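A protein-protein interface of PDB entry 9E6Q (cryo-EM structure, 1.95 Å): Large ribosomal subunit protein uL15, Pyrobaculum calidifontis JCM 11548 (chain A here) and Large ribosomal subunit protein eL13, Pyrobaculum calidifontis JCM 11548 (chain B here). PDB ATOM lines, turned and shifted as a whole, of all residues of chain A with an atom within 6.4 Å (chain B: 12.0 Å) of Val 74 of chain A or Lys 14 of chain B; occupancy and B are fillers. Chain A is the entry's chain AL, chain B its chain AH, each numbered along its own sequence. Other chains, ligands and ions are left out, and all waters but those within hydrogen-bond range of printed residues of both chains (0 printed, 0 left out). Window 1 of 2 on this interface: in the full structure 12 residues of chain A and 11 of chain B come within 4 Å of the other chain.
Hydrophobic or aromatic side chains of chain A that line the printed part of chain B: Val 74 and Leu 153.
Of the 12 printed residues of chain B, 5 touch a printed residue of chain A.
Printed residues of chain B that touch a printed residue of chain A: Ile 13, Lys 14, Ser 15, Gly 16 and Gly 17.
Among the printed residues, no Asp or Glu carboxylate lies within 4 Å of a Lys or Arg side-chain nitrogen of the other chain.
Of the printed residues of chain B, Val 74 of chain A touches Ile 13 (3.5 Å), Lys 14 (3.996 Å) and Gly 16 (3.9 Å).
Printed residues of chain A within 4 Å of Lys 14 of chain B: Ser 73 (3.4 Å), Val 74 (3.996 Å) and Glu 75 (3.0 Å).
No residue of chain B comes within 4 Å of Thr 71 of chain A.
Of chain B, only Lys 14 comes within 4 Å of Ser 73 of chain A.
Of the printed residues of chain B, Glu 75 of chain A touches Lys 14 (3.0 Å).
No residue of chain B comes within 4 Å of Trp 76 of chain A.
Of the printed residues of chain A, Ser 15 of chain B touches Asn 114 (3.5 Å).
Printed residues of chain A within 4 Å of Gly 17 of chain B: Leu 153 (3.5 Å).
Printed residues of chain B within 4 Å of Leu 153 of chain A: Gly 16 (3.2 Å) and Gly 17 (3.5 Å).
Arg 77 of chain A touches none of the printed residues of chain B.
The nearest printed residue of chain B that does not touch Val 74 of chain A is Ser 15 of chain B (5.1 Å).
Ser 73 of chain A touches Lys 14 of chain B (O to CA, 3.4 Å).
Val 74 of chain A touches Ile 13 of chain B (CG2 to O, 3.5 Å).
C of Val 74 of chain A touches O of Lys 14 of chain B, at 3.996 Å.
CA of Gly 16 of chain B touches CG1 of Val 74 of chain A, at 3.9 Å.
Asn 114 of chain A touches Gly 16 of chain B.
Gly 16 of chain B touches Leu 153 of chain A (O to CD2, 3.2 Å).
Gly 17 of chain B touches Leu 153 of chain A.
O of Lys 14 of chain B sits at hydrogen-bond distance from N of Glu 75 of chain A, at 3.0 Å.
The backbone carbonyl oxygen (O) of Ser 15 of chain B sits at hydrogen-bond distance from the side-chain amide nitrogen (ND2) of Asn 114 of chain A, at 3.5 Å.
OG of Ser 15 of chain B lies within hydrogen-bond range of N of Gly 17 of chain B, at 3.2 Å.
OG of Ser 15 of chain B is in hydrogen-bond range of O of Ser 12 of chain B, at 3.1 Å.
The backbone carbonyl oxygen (O) of Glu 75 of chain A is in hydrogen-bond range of the side-chain amide nitrogen (ND2) of Asn 114 of chain A (3.3 Å).
The side-chain hydroxyl of Ser 15 of chain B lies within hydrogen-bond range of the backbone carbonyl oxygen of Val 18 of chain B, at 3.3 Å.
OD1 of Asn 114 of chain A sits at hydrogen-bond distance from N of Arg 77 of chain A, at 2.7 Å.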
ATOM      1  N   GLU A  70     -39.367  20.413  -2.683  1.00  0.00           N
ATOM      2  CA  GLU A  70     -38.040  19.966  -2.273  1.00  0.00           C
ATOM      3  C   GLU A  70     -36.985  20.279  -3.321  1.00  0.00           C
ATOM      4  O   GLU A  70     -35.809  20.439  -2.981  1.00  0.00           O
ATOM      5  CB  GLU A  70     -38.053  18.470  -1.975  1.00  0.00           C
ATOM      6  CG  GLU A  70     -38.841  17.644  -2.970  1.00  0.00           C
ATOM      7  CD  GLU A  70     -39.222  16.279  -2.425  1.00  0.00           C
ATOM      8  OE1 GLU A  70     -39.620  16.203  -1.244  1.00  0.00           O
ATOM      9  OE2 GLU A  70     -39.134  15.286  -3.177  1.00  0.00           O
ATOM     10  N   THR A  71     -37.374  20.371  -4.590  1.00  0.00           N
ATOM     11  CA  THR A  71     -36.399  20.671  -5.626  1.00  0.00           C
ATOM     12  C   THR A  71     -35.898  22.106  -5.575  1.00  0.00           C
ATOM     13  O   THR A  71     -34.940  22.429  -6.278  1.00  0.00           O
ATOM     14  CB  THR A  71     -36.982  20.379  -7.006  1.00  0.00           C
ATOM     15  OG1 THR A  71     -38.115  21.224  -7.237  1.00  0.00           O
ATOM     16  CG2 THR A  71     -37.399  18.924  -7.105  1.00  0.00           C
ATOM     17  N   ILE A  72     -36.510  22.974  -4.774  1.00  0.00           N
ATOM     18  CA  ILE A  72     -36.032  24.345  -4.664  1.00  0.00           C
ATOM     19  C   ILE A  72     -35.699  24.658  -3.213  1.00  0.00           C
ATOM     20  O   ILE A  72     -35.553  25.825  -2.837  1.00  0.00           O
ATOM     21  CB  ILE A  72     -37.054  25.347  -5.227  1.00  0.00           C
ATOM     22  CG1 ILE A  72     -38.280  25.443  -4.321  1.00  0.00           C
ATOM     23  CG2 ILE A  72     -37.457  24.957  -6.632  1.00  0.00           C
ATOM     24  CD1 ILE A  72     -39.099  26.668  -4.558  1.00  0.00           C
ATOM     25  N   SER A  73     -35.550  23.625  -2.394  1.00  0.00           N
ATOM     26  CA  SER A  73     -35.249  23.785  -0.979  1.00  0.00           C
ATOM     27  C   SER A  73     -33.913  23.139  -0.655  1.00  0.00           C
ATOM     28  O   SER A  73     -33.631  22.021  -1.091  1.00  0.00           O
ATOM     29  CB  SER A  73     -36.346  23.172  -0.107  1.00  0.00           C
ATOM     30  OG  SER A  73     -37.607  23.712  -0.441  1.00  0.00           O
ATOM     31  N   VAL A  74     -33.095  23.849   0.117  1.00  0.00           N
ATOM     32  CA  VAL A  74     -31.813  23.310   0.543  1.00  0.00           C
ATOM     33  C   VAL A  74     -32.038  22.187   1.544  1.00  0.00           C
ATOM     34  O   VAL A  74     -32.845  22.310   2.474  1.00  0.00           O
ATOM     35  CB  VAL A  74     -30.934  24.421   1.141  1.00  0.00           C
ATOM     36  CG1 VAL A  74     -29.718  23.828   1.813  1.00  0.00           C
ATOM     37  CG2 VAL A  74     -30.530  25.404   0.071  1.00  0.00           C
ATOM     38  N   GLU A  75     -31.341  21.076   1.341  1.00  0.00           N
ATOM     39  CA  GLU A  75     -31.300  19.989   2.310  1.00  0.00           C
ATOM     40  C   GLU A  75     -30.115  20.234   3.237  1.00  0.00           C
ATOM     41  O   GLU A  75     -28.961  20.070   2.834  1.00  0.00           O
ATOM     42  CB  GLU A  75     -31.186  18.645   1.598  1.00  0.00           C
ATOM     43  CG  GLU A  75     -31.569  17.451   2.441  1.00  0.00           C
ATOM     44  CD  GLU A  75     -30.361  16.740   3.022  1.00  0.00           C
ATOM     45  OE1 GLU A  75     -29.238  17.262   2.881  1.00  0.00           O
ATOM     46  OE2 GLU A  75     -30.535  15.658   3.621  1.00  0.00           O
ATOM     47  N   TRP A  76     -30.400  20.637   4.472  1.00  0.00           N
ATOM     48  CA  TRP A  76     -29.358  21.044   5.405  1.00  0.00           C
ATOM     49  C   TRP A  76     -28.679  19.841   6.040  1.00  0.00           C
ATOM     50  O   TRP A  76     -29.323  18.838   6.348  1.00  0.00           O
ATOM     51  CB  TRP A  76     -29.944  21.936   6.493  1.00  0.00           C
ATOM     52  CG  TRP A  76     -30.475  23.217   5.972  1.00  0.00           C
ATOM     53  CD1 TRP A  76     -31.780  23.580   5.886  1.00  0.00           C
ATOM     54  CD2 TRP A  76     -29.718  24.314   5.460  1.00  0.00           C
ATOM     55  NE1 TRP A  76     -31.887  24.833   5.349  1.00  0.00           N
ATOM     56  CE2 TRP A  76     -30.635  25.307   5.079  1.00  0.00           C
ATOM     57  CE3 TRP A  76     -28.354  24.549   5.280  1.00  0.00           C
ATOM     58  CZ2 TRP A  76     -30.235  26.518   4.538  1.00  0.00           C
ATOM     59  CZ3 TRP A  76     -27.962  25.748   4.745  1.00  0.00           C
ATOM     60  CH2 TRP A  76     -28.899  26.721   4.380  1.00  0.00           C
ATOM     61  N   ARG A  77     -27.366  19.944   6.219  1.00  0.00           N
ATOM     62  CA  ARG A  77     -26.571  18.946   6.934  1.00  0.00           C
ATOM     63  C   ARG A  77     -25.732  19.669   7.976  1.00  0.00           C
ATOM     64  O   ARG A  77     -24.527  19.862   7.793  1.00  0.00           O
ATOM     65  CB  ARG A  77     -25.688  18.143   5.982  1.00  0.00           C
ATOM     66  CG  ARG A  77     -26.349  17.751   4.686  1.00  0.00           C
ATOM     67  CD  ARG A  77     -25.667  16.563   4.003  1.00  0.00           C
ATOM     68  NE  ARG A  77     -25.752  15.326   4.775  1.00  0.00           N
ATOM     69  CZ  ARG A  77     -24.868  14.930   5.683  1.00  0.00           C
ATOM     70  NH1 ARG A  77     -23.769  15.623   5.927  1.00  0.00           N
ATOM     71  NH2 ARG A  77     -25.087  13.803   6.352  1.00  0.00           N
ATOM     72  N   ASN A 114     -22.984  21.825   5.566  1.00  0.00           N
ATOM     73  CA  ASN A 114     -23.302  23.128   4.997  1.00  0.00           C
ATOM     74  C   ASN A 114     -23.955  24.060   6.011  1.00  0.00           C
ATOM     75  O   ASN A 114     -24.591  25.038   5.616  1.00  0.00           O
ATOM     76  CB  ASN A 114     -24.194  22.966   3.766  1.00  0.00           C
ATOM     77  CG  ASN A 114     -25.447  22.165   4.051  1.00  0.00           C
ATOM     78  OD1 ASN A 114     -25.806  21.936   5.201  1.00  0.00           O
ATOM     79  ND2 ASN A 114     -26.114  21.728   2.997  1.00  0.00           N
ATOM     80  N   LEU A 153     -23.358  30.739  -1.410  1.00  0.00           N
ATOM     81  CA  LEU A 153     -23.751  29.620  -2.259  1.00  0.00           C
ATOM     82  C   LEU A 153     -24.094  30.110  -3.656  1.00  0.00           C
ATOM     83  O   LEU A 153     -25.261  30.379  -3.955  1.00  0.00           O
ATOM     84  CB  LEU A 153     -24.948  28.874  -1.666  1.00  0.00           C
ATOM     85  CG  LEU A 153     -24.700  28.086  -0.382  1.00  0.00           C
ATOM     86  CD1 LEU A 153     -25.998  27.565   0.210  1.00  0.00           C
ATOM     87  CD2 LEU A 153     -23.752  26.956  -0.667  1.00  0.00           C
ATOM     88  N   VAL B   9     -20.095  16.859 -11.040  1.00  0.00           N
ATOM     89  CA  VAL B   9     -21.519  16.560 -10.862  1.00  0.00           C
ATOM     90  C   VAL B   9     -22.287  17.871 -10.759  1.00  0.00           C
ATOM     91  O   VAL B   9     -21.870  18.767 -10.007  1.00  0.00           O
ATOM     92  CB  VAL B   9     -21.727  15.700  -9.617  1.00  0.00           C
ATOM     93  CG1 VAL B   9     -23.198  15.559  -9.310  1.00  0.00           C
ATOM     94  CG2 VAL B   9     -21.094  14.348  -9.801  1.00  0.00           C
ATOM     95  N   PRO B  10     -23.386  18.042 -11.490  1.00  0.00           N
ATOM     96  CA  PRO B  10     -24.148  19.292 -11.398  1.00  0.00           C
ATOM     97  C   PRO B  10     -24.586  19.577  -9.970  1.00  0.00           C
ATOM     98  O   PRO B  10     -25.132  18.715  -9.285  1.00  0.00           O
ATOM     99  CB  PRO B  10     -25.349  19.051 -12.314  1.00  0.00           C
ATOM    100  CG  PRO B  10     -25.042  17.870 -13.110  1.00  0.00           C
ATOM    101  CD  PRO B  10     -23.890  17.138 -12.534  1.00  0.00           C
ATOM    102  N   ARG B  11     -24.347  20.805  -9.529  1.00  0.00           N
ATOM    103  CA  ARG B  11     -24.639  21.214  -8.161  1.00  0.00           C
ATOM    104  C   ARG B  11     -26.093  21.651  -8.069  1.00  0.00           C
ATOM    105  O   ARG B  11     -26.455  22.721  -8.561  1.00  0.00           O
ATOM    106  CB  ARG B  11     -23.705  22.343  -7.746  1.00  0.00           C
ATOM    107  CG  ARG B  11     -23.757  22.686  -6.282  1.00  0.00           C
ATOM    108  CD  ARG B  11     -22.871  23.873  -5.968  1.00  0.00           C
ATOM    109  NE  ARG B  11     -23.488  25.138  -6.346  1.00  0.00           N
ATOM    110  CZ  ARG B  11     -22.819  26.262  -6.553  1.00  0.00           C
ATOM    111  NH1 ARG B  11     -21.503  26.312  -6.445  1.00  0.00           N
ATOM    112  NH2 ARG B  11     -23.487  27.366  -6.871  1.00  0.00           N
ATOM    113  N   SER B  12     -26.927  20.837  -7.436  1.00  0.00           N
ATOM    114  CA  SER B  12     -28.330  21.182  -7.303  1.00  0.00           C
ATOM    115  C   SER B  12     -28.534  22.185  -6.173  1.00  0.00           C
ATOM    116  O   SER B  12     -27.679  22.368  -5.305  1.00  0.00           O
ATOM    117  CB  SER B  12     -29.176  19.937  -7.050  1.00  0.00           C
ATOM    118  OG  SER B  12     -28.836  19.332  -5.823  1.00  0.00           O
ATOM    119  N   ILE B  13     -29.685  22.853  -6.206  1.00  0.00           N
ATOM    120  CA  ILE B  13     -30.082  23.704  -5.090  1.00  0.00           C
ATOM    121  C   ILE B  13     -30.228  22.874  -3.823  1.00  0.00           C
ATOM    122  O   ILE B  13     -29.887  23.322  -2.726  1.00  0.00           O
ATOM    123  CB  ILE B  13     -31.380  24.456  -5.428  1.00  0.00           C
ATOM    124  CG1 ILE B  13     -31.199  25.279  -6.699  1.00  0.00           C
ATOM    125  CG2 ILE B  13     -31.808  25.339  -4.271  1.00  0.00           C
ATOM    126  CD1 ILE B  13     -32.500  25.697  -7.330  1.00  0.00           C
ATOM    127  N   LYS B  14     -30.733  21.650  -3.962  1.00  0.00           N
ATOM    128  CA  LYS B  14     -30.926  20.769  -2.816  1.00  0.00           C
ATOM    129  C   LYS B  14     -29.614  20.441  -2.117  1.00  0.00           C
ATOM    130  O   LYS B  14     -29.602  20.184  -0.910  1.00  0.00           O
ATOM    131  CB  LYS B  14     -31.618  19.487  -3.278  1.00  0.00           C
ATOM    132  CG  LYS B  14     -32.240  18.670  -2.172  1.00  0.00           C
ATOM    133  CD  LYS B  14     -33.021  17.490  -2.731  1.00  0.00           C
ATOM    134  CE  LYS B  14     -32.154  16.627  -3.629  1.00  0.00           C
ATOM    135  NZ  LYS B  14     -32.842  15.377  -4.064  1.00  0.00           N
ATOM    136  N   SER B  15     -28.501  20.447  -2.851  1.00  0.00           N
ATOM    137  CA  SER B  15     -27.226  20.043  -2.272  1.00  0.00           C
ATOM    138  C   SER B  15     -26.720  21.043  -1.241  1.00  0.00           C
ATOM    139  O   SER B  15     -26.031  20.654  -0.293  1.00  0.00           O
ATOM    140  CB  SER B  15     -26.190  19.850  -3.377  1.00  0.00           C
ATOM    141  OG  SER B  15     -25.433  21.026  -3.577  1.00  0.00           O
ATOM    142  N   GLY B  16     -27.038  22.323  -1.402  1.00  0.00           N
ATOM    143  CA  GLY B  16     -26.554  23.315  -0.466  1.00  0.00           C
ATOM    144  C   GLY B  16     -25.078  23.617  -0.565  1.00  0.00           C
ATOM    145  O   GLY B  16     -24.476  24.038   0.423  1.00  0.00           O
ATOM    146  N   GLY B  17     -24.469  23.402  -1.728  1.00  0.00           N
ATOM    147  CA  GLY B  17     -23.083  23.748  -1.956  1.00  0.00           C
ATOM    148  C   GLY B  17     -22.121  22.583  -1.979  1.00  0.00           C
ATOM    149  O   GLY B  17     -20.962  22.776  -2.355  1.00  0.00           O
ATOM    150  N   VAL B  18     -22.549  21.390  -1.595  1.00  0.00           N
ATOM    151  CA  VAL B  18     -21.668  20.229  -1.613  1.00  0.00           C
ATOM    152  C   VAL B  18     -21.542  19.721  -3.042  1.00  0.00           C
ATOM    153  O   VAL B  18     -22.548  19.483  -3.718  1.00  0.00           O
ATOM    154  CB  VAL B  18     -22.195  19.134  -0.677  1.00  0.00           C
ATOM    155  CG1 VAL B  18     -21.189  18.007  -0.572  1.00  0.00           C
ATOM    156  CG2 VAL B  18     -22.489  19.713   0.686  1.00  0.00           C
ATOM    157  N   THR B  19     -20.305  19.550  -3.503  1.00  0.00           N
ATOM    158  CA  THR B  19     -20.019  19.157  -4.874  1.00  0.00           C
ATOM    159  C   THR B  19     -19.122  17.928  -4.887  1.00  0.00           C
ATOM    160  O   THR B  19     -18.415  17.641  -3.921  1.00  0.00           O
ATOM    161  CB  THR B  19     -19.338  20.282  -5.665  1.00  0.00           C
ATOM    162  OG1 THR B  19     -18.065  20.576  -5.079  1.00  0.00           O
ATOM    163  CG2 THR B  19     -20.185  21.530  -5.665  1.00  0.00           C
ATOM    164  N   LYS B  20     -19.158  17.205  -6.005  1.00  0.00           N
ATOM    165  CA  LYS B  20     -18.336  16.020  -6.187  1.00  0.00           C
ATOM    166  C   LYS B  20     -18.019  15.856  -7.664  1.00  0.00           C
ATOM    167  O   LYS B  20     -18.600  16.516  -8.523  1.00  0.00           O
ATOM    168  CB  LYS B  20     -19.026  14.774  -5.626  1.00  0.00           C
ATOM    169  CG  LYS B  20     -20.536  14.829  -5.700  1.00  0.00           C
ATOM    170  CD  LYS B  20     -21.184  13.473  -5.476  1.00  0.00           C
ATOM    171  CE  LYS B  20     -20.543  12.377  -6.297  1.00  0.00           C
ATOM    172  NZ  LYS B  20     -21.255  11.078  -6.128  1.00  0.00           N
